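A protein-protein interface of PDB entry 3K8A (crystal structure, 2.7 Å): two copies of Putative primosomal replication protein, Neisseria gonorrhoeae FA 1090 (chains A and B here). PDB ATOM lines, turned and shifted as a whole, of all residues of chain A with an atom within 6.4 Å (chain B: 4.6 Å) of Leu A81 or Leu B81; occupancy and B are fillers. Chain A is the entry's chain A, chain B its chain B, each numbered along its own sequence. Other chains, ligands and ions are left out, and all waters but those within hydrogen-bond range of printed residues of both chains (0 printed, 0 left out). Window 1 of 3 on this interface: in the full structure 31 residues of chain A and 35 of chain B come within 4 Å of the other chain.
N of Leu A81 lies within hydrogen-bond range of OD1 of Asn A8 (2.7 Å). The backbone NH (N) of His A38 lies within hydrogen-bond range of the backbone carbonyl oxygen (O) of Leu A53 (2.6 Å). The backbone carbonyl oxygen of Phe A80 lies within hydrogen-bond range of the backbone NH of Arg A94. The backbone NH (N) of Met A92 lies within hydrogen-bond range of the backbone carbonyl oxygen (O) of Ala A82. The backbone NH (N) of Leu B81 lies within hydrogen-bond range of the side-chain amide oxygen (OD1) of Asn B8 (2.9 Å). O of Ala B82 lies within hydrogen-bond range of N of Met B92.
Among the printed residues, pairs that only touch across the chains: His A38 with Asn B8, Leu A9 with Val B10, Leu A53 with Leu B81, Phe A80 with Val B51, Val A51 with Leu B81, Leu A81 with Val B51, Leu A12 with Asn B8, Val A51 with Ala B82, Leu A81 with Leu B53, Gln A52 with Ala B82, Leu A81 with Leu B81, Val A51 with Phe B80, Ala A82 with Val B51, Pro A91 with Leu B53 and Gln A83 with Leu B53.
Leu A81 touches just these residues of chain B: Val B51 (3.5 Å), Leu B53 (3.7 Å) and Leu B81 (3.8 Å). Leu B81 touches just these residues of chain A: Val A51, Leu A53 and Leu A81. Of the printed residues of chain B, Gln A52 touches Ala B82 (3.7 Å). Of the printed residues of chain B, His A38 touches Asn B8 (3.2 Å). Printed residues of chain B within 4 Å of Val A51: Phe B80, Leu B81 and Ala B82. Of the printed residues of chain A, Ala B82 touches Val A51 and Gln A52. The nearest residue of chain B that does not touch Leu A81 is Val B10 (4.1 Å). The nearest residue of chain A that does not touch Leu B81 is Ile A55 (4.1 Å). The nearest printed residue of chain A that does not touch Val B51 is Asn A8 (4.1 Å).
Hydrophobic or aromatic side chains of chain B that line the printed part of chain A: Val B10, Val B51, Leu B53, Phe B80, Leu B81 and Ala B82. Of the 18 printed residues of chain A, 11 touch a printed residue of chain B. Among the printed residues, 15 pairs touch across the chains. Among the printed residues, no Asp or Glu carboxylate lies within 4 Å of a Lys or Arg side-chain nitrogen of the other chain.
Val A51 touches Phe B80, and with the chains exchanged Phe A80 touches Val B51. Val A51 touches Leu B81, and with the chains exchanged Leu A81 touches Val B51. Val A51 touches Ala B82, and with the chains exchanged Ala A82 touches Val B51. Leu A53 touches Leu B81, and with the chains exchanged Leu A81 touches Leu B53. Positions printed for both chains: 8, 10, 51, 53, 55, 80, 81, 82, 92 and 93. Of the 15 pairs that touch across the chains among the printed residues, 9 have their exchanged pair printed and touching as well.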
ATOM      1  N   ASN A   8      25.940  31.135 -16.893  1.00  0.00           N
ATOM      2  CA  ASN A   8      25.283  29.923 -17.297  1.00  0.00           C
ATOM      3  C   ASN A   8      26.324  28.992 -17.954  1.00  0.00           C
ATOM      4  O   ASN A   8      26.436  28.963 -19.168  1.00  0.00           O
ATOM      5  CB  ASN A   8      24.114  30.252 -18.218  1.00  0.00           C
ATOM      6  CG  ASN A   8      23.154  29.068 -18.400  1.00  0.00           C
ATOM      7  OD1 ASN A   8      23.577  27.887 -18.471  1.00  0.00           O
ATOM      8  ND2 ASN A   8      21.852  29.377 -18.483  1.00  0.00           N
ATOM      9  N   LEU A   9      27.126  28.289 -17.157  1.00  0.00           N
ATOM     10  CA  LEU A   9      28.210  27.477 -17.727  1.00  0.00           C
ATOM     11  C   LEU A   9      28.152  25.985 -17.424  1.00  0.00           C
ATOM     12  O   LEU A   9      28.349  25.574 -16.291  1.00  0.00           O
ATOM     13  CB  LEU A   9      29.580  28.025 -17.328  1.00  0.00           C
ATOM     14  CG  LEU A   9      30.173  28.960 -18.392  1.00  0.00           C
ATOM     15  CD1 LEU A   9      30.856  30.200 -17.763  1.00  0.00           C
ATOM     16  CD2 LEU A   9      31.103  28.211 -19.424  1.00  0.00           C
ATOM     17  N   VAL A  10      27.881  25.180 -18.436  1.00  0.00           N
ATOM     18  CA  VAL A  10      28.085  23.730 -18.310  1.00  0.00           C
ATOM     19  C   VAL A  10      29.318  23.211 -19.051  1.00  0.00           C
ATOM     20  O   VAL A  10      29.501  23.528 -20.202  1.00  0.00           O
ATOM     21  CB  VAL A  10      26.863  22.962 -18.823  1.00  0.00           C
ATOM     22  CG1 VAL A  10      26.913  21.564 -18.349  1.00  0.00           C
ATOM     23  CG2 VAL A  10      25.615  23.619 -18.292  1.00  0.00           C
ATOM     24  N   LEU A  12      30.513  19.358 -19.761  1.00  0.00           N
ATOM     25  CA  LEU A  12      30.094  17.977 -19.588  1.00  0.00           C
ATOM     26  C   LEU A  12      30.851  17.107 -20.551  1.00  0.00           C
ATOM     27  O   LEU A  12      31.000  17.447 -21.722  1.00  0.00           O
ATOM     28  CB  LEU A  12      28.602  17.861 -19.885  1.00  0.00           C
ATOM     29  CG  LEU A  12      27.928  16.537 -19.535  1.00  0.00           C
ATOM     30  CD1 LEU A  12      27.739  16.366 -17.996  1.00  0.00           C
ATOM     31  CD2 LEU A  12      26.595  16.414 -20.288  1.00  0.00           C
ATOM     32  N   HIS A  38      25.444  10.678 -20.247  1.00  0.00           N
ATOM     33  CA  HIS A  38      26.551  10.888 -19.351  1.00  0.00           C
ATOM     34  C   HIS A  38      26.498   9.939 -18.166  1.00  0.00           C
ATOM     35  O   HIS A  38      25.434   9.491 -17.753  1.00  0.00           O
ATOM     36  CB  HIS A  38      26.555  12.317 -18.858  1.00  0.00           C
ATOM     37  CG  HIS A  38      27.539  12.546 -17.769  1.00  0.00           C
ATOM     38  ND1 HIS A  38      27.236  12.328 -16.442  1.00  0.00           N
ATOM     39  CD2 HIS A  38      28.837  12.936 -17.809  1.00  0.00           C
ATOM     40  CE1 HIS A  38      28.302  12.602 -15.708  1.00  0.00           C
ATOM     41  NE2 HIS A  38      29.289  12.961 -16.513  1.00  0.00           N
ATOM     42  N   VAL A  51      26.461   8.826 -11.052  1.00  0.00           N
ATOM     43  CA  VAL A  51      25.609   9.815 -11.701  1.00  0.00           C
ATOM     44  C   VAL A  51      25.211   9.393 -13.127  1.00  0.00           C
ATOM     45  O   VAL A  51      26.071   9.076 -13.935  1.00  0.00           O
ATOM     46  CB  VAL A  51      26.303  11.196 -11.761  1.00  0.00           C
ATOM     47  CG1 VAL A  51      25.489  12.146 -12.559  1.00  0.00           C
ATOM     48  CG2 VAL A  51      26.522  11.740 -10.360  1.00  0.00           C
ATOM     49  N   GLN A  52      23.909   9.397 -13.405  1.00  0.00           N
ATOM     50  CA  GLN A  52      23.350   9.105 -14.715  1.00  0.00           C
ATOM     51  C   GLN A  52      22.700  10.362 -15.257  1.00  0.00           C
ATOM     52  O   GLN A  52      22.028  11.070 -14.533  1.00  0.00           O
ATOM     53  CB  GLN A  52      22.252   8.052 -14.626  1.00  0.00           C
ATOM     54  CG  GLN A  52      22.678   6.658 -14.189  1.00  0.00           C
ATOM     55  CD  GLN A  52      21.619   5.605 -14.549  1.00  0.00           C
ATOM     56  OE1 GLN A  52      21.321   5.378 -15.731  1.00  0.00           O
ATOM     57  NE2 GLN A  52      21.047   4.968 -13.530  1.00  0.00           N
ATOM     58  N   LEU A  53      22.877  10.631 -16.543  1.00  0.00           N
ATOM     59  CA  LEU A  53      22.253  11.796 -17.147  1.00  0.00           C
ATOM     60  C   LEU A  53      22.093  11.680 -18.657  1.00  0.00           C
ATOM     61  O   LEU A  53      23.058  11.433 -19.381  1.00  0.00           O
ATOM     62  CB  LEU A  53      23.044  13.045 -16.803  1.00  0.00           C
ATOM     63  CG  LEU A  53      22.547  14.315 -17.457  1.00  0.00           C
ATOM     64  CD1 LEU A  53      21.200  14.665 -16.915  1.00  0.00           C
ATOM     65  CD2 LEU A  53      23.526  15.383 -17.145  1.00  0.00           C
ATOM     66  N   ILE A  55      20.527  13.993 -21.708  1.00  0.00           N
ATOM     67  CA  ILE A  55      20.118  15.380 -21.918  1.00  0.00           C
ATOM     68  C   ILE A  55      20.169  15.743 -23.405  1.00  0.00           C
ATOM     69  O   ILE A  55      21.187  15.528 -24.061  1.00  0.00           O
ATOM     70  CB  ILE A  55      21.032  16.337 -21.091  1.00  0.00           C
ATOM     71  CG1 ILE A  55      20.442  17.751 -20.978  1.00  0.00           C
ATOM     72  CG2 ILE A  55      22.448  16.377 -21.657  1.00  0.00           C
ATOM     73  CD1 ILE A  55      21.257  18.676 -20.081  1.00  0.00           C
ATOM     74  N   GLY A  79      28.967  24.800 -22.717  1.00  0.00           N
ATOM     75  CA  GLY A  79      27.876  25.659 -23.172  1.00  0.00           C
ATOM     76  C   GLY A  79      27.012  26.239 -22.075  1.00  0.00           C
ATOM     77  O   GLY A  79      27.487  26.474 -20.981  1.00  0.00           O
ATOM     78  N   PHE A  80      25.738  26.464 -22.389  1.00  0.00           N
ATOM     79  CA  PHE A  80      24.763  26.896 -21.404  1.00  0.00           C
ATOM     80  C   PHE A  80      23.435  26.124 -21.472  1.00  0.00           C
ATOM     81  O   PHE A  80      23.080  25.554 -22.489  1.00  0.00           O
ATOM     82  CB  PHE A  80      24.529  28.409 -21.489  1.00  0.00           C
ATOM     83  CG  PHE A  80      23.960  28.877 -22.811  1.00  0.00           C
ATOM     84  CD1 PHE A  80      22.607  28.722 -23.102  1.00  0.00           C
ATOM     85  CD2 PHE A  80      24.768  29.497 -23.755  1.00  0.00           C
ATOM     86  CE1 PHE A  80      22.073  29.171 -24.320  1.00  0.00           C
ATOM     87  CE2 PHE A  80      24.239  29.935 -24.964  1.00  0.00           C
ATOM     88  CZ  PHE A  80      22.885  29.772 -25.242  1.00  0.00           C
ATOM     89  N   LEU A  81      22.711  26.129 -20.360  1.00  0.00           N
ATOM     90  CA  LEU A  81      21.461  25.399 -20.201  1.00  0.00           C
ATOM     91  C   LEU A  81      20.265  26.260 -20.516  1.00  0.00           C
ATOM     92  O   LEU A  81      20.239  27.437 -20.168  1.00  0.00           O
ATOM     93  CB  LEU A  81      21.339  24.937 -18.761  1.00  0.00           C
ATOM     94  CG  LEU A  81      22.119  23.670 -18.482  1.00  0.00           C
ATOM     95  CD1 LEU A  81      22.253  23.413 -16.968  1.00  0.00           C
ATOM     96  CD2 LEU A  81      21.412  22.521 -19.186  1.00  0.00           C
ATOM     97  N   ALA A  82      19.252  25.666 -21.133  1.00  0.00           N
ATOM     98  CA  ALA A  82      18.069  26.424 -21.572  1.00  0.00           C
ATOM     99  C   ALA A  82      16.897  25.492 -21.769  1.00  0.00           C
ATOM    100  O   ALA A  82      17.074  24.296 -21.914  1.00  0.00           O
ATOM    101  CB  ALA A  82      18.363  27.187 -22.867  1.00  0.00           C
ATOM    102  N   GLN A  83      15.690  26.023 -21.762  1.00  0.00           N
ATOM    103  CA  GLN A  83      14.552  25.168 -21.995  1.00  0.00           C
ATOM    104  C   GLN A  83      14.187  25.144 -23.455  1.00  0.00           C
ATOM    105  O   GLN A  83      13.756  26.154 -23.996  1.00  0.00           O
ATOM    106  CB  GLN A  83      13.375  25.611 -21.155  1.00  0.00           C
ATOM    107  CG  GLN A  83      13.714  25.504 -19.689  1.00  0.00           C
ATOM    108  CD  GLN A  83      12.513  25.263 -18.842  1.00  0.00           C
ATOM    109  OE1 GLN A  83      11.693  26.161 -18.643  1.00  0.00           O
ATOM    110  NE2 GLN A  83      12.384  24.045 -18.338  1.00  0.00           N
ATOM    111  N   PRO A  91      14.937  21.058 -19.785  1.00  0.00           N
ATOM    112  CA  PRO A  91      16.152  21.766 -20.128  1.00  0.00           C
ATOM    113  C   PRO A  91      16.943  21.078 -21.226  1.00  0.00           C
ATOM    114  O   PRO A  91      16.825  19.883 -21.441  1.00  0.00           O
ATOM    115  CB  PRO A  91      16.952  21.756 -18.816  1.00  0.00           C
ATOM    116  CG  PRO A  91      16.180  20.947 -17.849  1.00  0.00           C
ATOM    117  CD  PRO A  91      15.150  20.198 -18.612  1.00  0.00           C
ATOM    118  N   MET A  92      17.762  21.855 -21.903  1.00  0.00           N
ATOM    119  CA  MET A  92      18.567  21.352 -22.985  1.00  0.00           C
ATOM    120  C   MET A  92      19.931  22.033 -22.966  1.00  0.00           C
ATOM    121  O   MET A  92      20.067  23.135 -22.460  1.00  0.00           O
ATOM    122  CB  MET A  92      17.864  21.633 -24.291  1.00  0.00           C
ATOM    123  CG  MET A  92      18.796  21.831 -25.427  1.00  0.00           C
ATOM    124  SD  MET A  92      17.967  22.702 -26.762  1.00  0.00           S
ATOM    125  CE  MET A  92      17.497  24.232 -25.932  1.00  0.00           C
ATOM    126  N   LEU A  93      20.946  21.365 -23.488  1.00  0.00           N
ATOM    127  CA  LEU A  93      22.265  21.964 -23.541  1.00  0.00           C
ATOM    128  C   LEU A  93      22.604  22.581 -24.925  1.00  0.00           C
ATOM    129  O   LEU A  93      22.572  21.909 -25.960  1.00  0.00           O
ATOM    130  CB  LEU A  93      23.305  20.938 -23.117  1.00  0.00           C
ATOM    131  CG  LEU A  93      24.754  21.414 -23.114  1.00  0.00           C
ATOM    132  CD1 LEU A  93      24.931  22.709 -22.334  1.00  0.00           C
ATOM    133  CD2 LEU A  93      25.608  20.344 -22.534  1.00  0.00           C
ATOM    134  N   ARG A  94      22.910  23.873 -24.928  1.00  0.00           N
ATOM    135  CA  ARG A  94      23.289  24.586 -26.139  1.00  0.00           C
ATOM    136  C   ARG A  94      24.789  24.733 -26.196  1.00  0.00           C
ATOM    137  O   ARG A  94      25.369  25.645 -25.602  1.00  0.00           O
ATOM    138  CB  ARG A  94      22.684  25.967 -26.130  1.00  0.00           C
ATOM    139  CG  ARG A  94      21.215  25.930 -25.922  1.00  0.00           C
ATOM    140  CD  ARG A  94      20.480  26.237 -27.190  1.00  0.00           C
ATOM    141  NE  ARG A  94      19.321  27.044 -26.867  1.00  0.00           N
ATOM    142  CZ  ARG A  94      19.230  28.351 -27.083  1.00  0.00           C
ATOM    143  NH1 ARG A  94      20.210  29.015 -27.675  1.00  0.00           N
ATOM    144  NH2 ARG A  94      18.130  28.984 -26.729  1.00  0.00           N
ATOM    145  N   ASN B   8      31.605  16.882 -15.107  1.00  0.00           N
ATOM    146  CA  ASN B   8      30.233  17.316 -14.973  1.00  0.00           C
ATOM    147  C   ASN B   8      30.177  18.626 -14.161  1.00  0.00           C
ATOM    148  O   ASN B   8      30.064  18.594 -12.938  1.00  0.00           O
ATOM    149  CB  ASN B   8      29.407  16.202 -14.340  1.00  0.00           C
ATOM    150  CG  ASN B   8      27.896  16.443 -14.455  1.00  0.00           C
ATOM    151  OD1 ASN B   8      27.411  17.586 -14.386  1.00  0.00           O
ATOM    152  ND2 ASN B   8      27.147  15.361 -14.606  1.00  0.00           N
ATOM    153  N   VAL B  10      28.386  22.398 -13.768  1.00  0.00           N
ATOM    154  CA  VAL B  10      27.522  23.567 -13.942  1.00  0.00           C
ATOM    155  C   VAL B  10      27.879  24.686 -12.968  1.00  0.00           C
ATOM    156  O   VAL B  10      27.984  24.449 -11.784  1.00  0.00           O
ATOM    157  CB  VAL B  10      26.042  23.218 -13.679  1.00  0.00           C
ATOM    158  CG1 VAL B  10      25.160  24.258 -14.271  1.00  0.00           C
ATOM    159  CG2 VAL B  10      25.703  21.878 -14.286  1.00  0.00           C
ATOM    160  N   VAL B  51      17.767  33.805 -22.633  1.00  0.00           N
ATOM    161  CA  VAL B  51      17.680  32.426 -22.175  1.00  0.00           C
ATOM    162  C   VAL B  51      16.867  32.324 -20.878  1.00  0.00           C
ATOM    163  O   VAL B  51      17.155  33.018 -19.912  1.00  0.00           O
ATOM    164  CB  VAL B  51      19.084  31.869 -21.919  1.00  0.00           C
ATOM    165  CG1 VAL B  51      19.002  30.602 -21.134  1.00  0.00           C
ATOM    166  CG2 VAL B  51      19.821  31.642 -23.243  1.00  0.00           C
ATOM    167  N   LEU B  53      15.292  29.567 -18.018  1.00  0.00           N
ATOM    168  CA  LEU B  53      15.528  28.242 -17.501  1.00  0.00           C
ATOM    169  C   LEU B  53      15.001  28.121 -16.078  1.00  0.00           C
ATOM    170  O   LEU B  53      15.327  28.930 -15.210  1.00  0.00           O
ATOM    171  CB  LEU B  53      17.021  27.937 -17.523  1.00  0.00           C
ATOM    172  CG  LEU B  53      17.436  26.667 -16.799  1.00  0.00           C
ATOM    173  CD1 LEU B  53      17.078  25.480 -17.636  1.00  0.00           C
ATOM    174  CD2 LEU B  53      18.903  26.694 -16.526  1.00  0.00           C
ATOM    175  N   ILE B  55      14.859  25.074 -13.214  1.00  0.00           N
ATOM    176  CA  ILE B  55      15.478  23.776 -12.971  1.00  0.00           C
ATOM    177  C   ILE B  55      15.408  23.355 -11.502  1.00  0.00           C
ATOM    178  O   ILE B  55      15.819  24.097 -10.614  1.00  0.00           O
ATOM    179  CB  ILE B  55      16.941  23.787 -13.451  1.00  0.00           C
ATOM    180  CG1 ILE B  55      17.483  22.369 -13.654  1.00  0.00           C
ATOM    181  CG2 ILE B  55      17.834  24.594 -12.508  1.00  0.00           C
ATOM    182  CD1 ILE B  55      18.912  22.346 -14.224  1.00  0.00           C
ATOM    183  N   PHE B  80      26.742  19.642 -10.292  1.00  0.00           N
ATOM    184  CA  PHE B  80      26.685  18.793 -11.456  1.00  0.00           C
ATOM    185  C   PHE B  80      25.259  18.329 -11.713  1.00  0.00           C
ATOM    186  O   PHE B  80      24.454  18.239 -10.797  1.00  0.00           O
ATOM    187  CB  PHE B  80      27.612  17.607 -11.272  1.00  0.00           C
ATOM    188  CG  PHE B  80      27.354  16.854 -10.020  1.00  0.00           C
ATOM    189  CD1 PHE B  80      28.125  17.075  -8.887  1.00  0.00           C
ATOM    190  CD2 PHE B  80      26.314  15.937  -9.954  1.00  0.00           C
ATOM    191  CE1 PHE B  80      27.871  16.395  -7.743  1.00  0.00           C
ATOM    192  CE2 PHE B  80      26.063  15.237  -8.802  1.00  0.00           C
ATOM    193  CZ  PHE B  80      26.832  15.465  -7.696  1.00  0.00           C
ATOM    194  N   LEU B  81      24.972  18.045 -12.980  1.00  0.00           N
ATOM    195  CA  LEU B  81      23.649  17.644 -13.435  1.00  0.00           C
ATOM    196  C   LEU B  81      23.428  16.173 -13.260  1.00  0.00           C
ATOM    197  O   LEU B  81      24.353  15.378 -13.398  1.00  0.00           O
ATOM    198  CB  LEU B  81      23.477  17.989 -14.909  1.00  0.00           C
ATOM    199  CG  LEU B  81      23.291  19.482 -15.168  1.00  0.00           C
ATOM    200  CD1 LEU B  81      23.326  19.791 -16.663  1.00  0.00           C
ATOM    201  CD2 LEU B  81      21.988  19.990 -14.523  1.00  0.00           C
ATOM    202  N   ALA B  82      22.187  15.807 -12.967  1.00  0.00           N
ATOM    203  CA  ALA B  82      21.821  14.392 -12.818  1.00  0.00           C
ATOM    204  C   ALA B  82      20.311  14.202 -12.935  1.00  0.00           C
ATOM    205  O   ALA B  82      19.531  15.123 -12.704  1.00  0.00           O
ATOM    206  CB  ALA B  82      22.343  13.831 -11.496  1.00  0.00           C
ATOM    207  N   MET B  92      18.333  17.429 -12.881  1.00  0.00           N
ATOM    208  CA  MET B  92      18.349  18.367 -11.782  1.00  0.00           C
ATOM    209  C   MET B  92      19.775  18.768 -11.435  1.00  0.00           C
ATOM    210  O   MET B  92      20.721  18.086 -11.786  1.00  0.00           O
ATOM    211  CB  MET B  92      17.719  17.740 -10.560  1.00  0.00           C
ATOM    212  CG  MET B  92      18.587  16.677  -9.968  1.00  0.00           C
ATOM    213  SD  MET B  92      18.173  16.544  -8.250  1.00  0.00           S
ATOM    214  CE  MET B  92      17.869  18.270  -7.867  1.00  0.00           C
ATOM    215  N   LEU B  93      19.911  19.878 -10.732  1.00  0.00           N
ATOM    216  CA  LEU B  93      21.198  20.336 -10.282  1.00  0.00           C
ATOM    217  C   LEU B  93      21.456  19.977  -8.803  1.00  0.00           C
ATOM    218  O   LEU B  93      20.686  20.342  -7.903  1.00  0.00           O
ATOM    219  CB  LEU B  93      21.284  21.836 -10.478  1.00  0.00           C
ATOM    220  CG  LEU B  93      22.640  22.424 -10.123  1.00  0.00           C
ATOM    221  CD1 LEU B  93      23.742  21.756 -10.928  1.00  0.00           C
ATOM    222  CD2 LEU B  93      22.626  23.910 -10.347  1.00  0.00           C
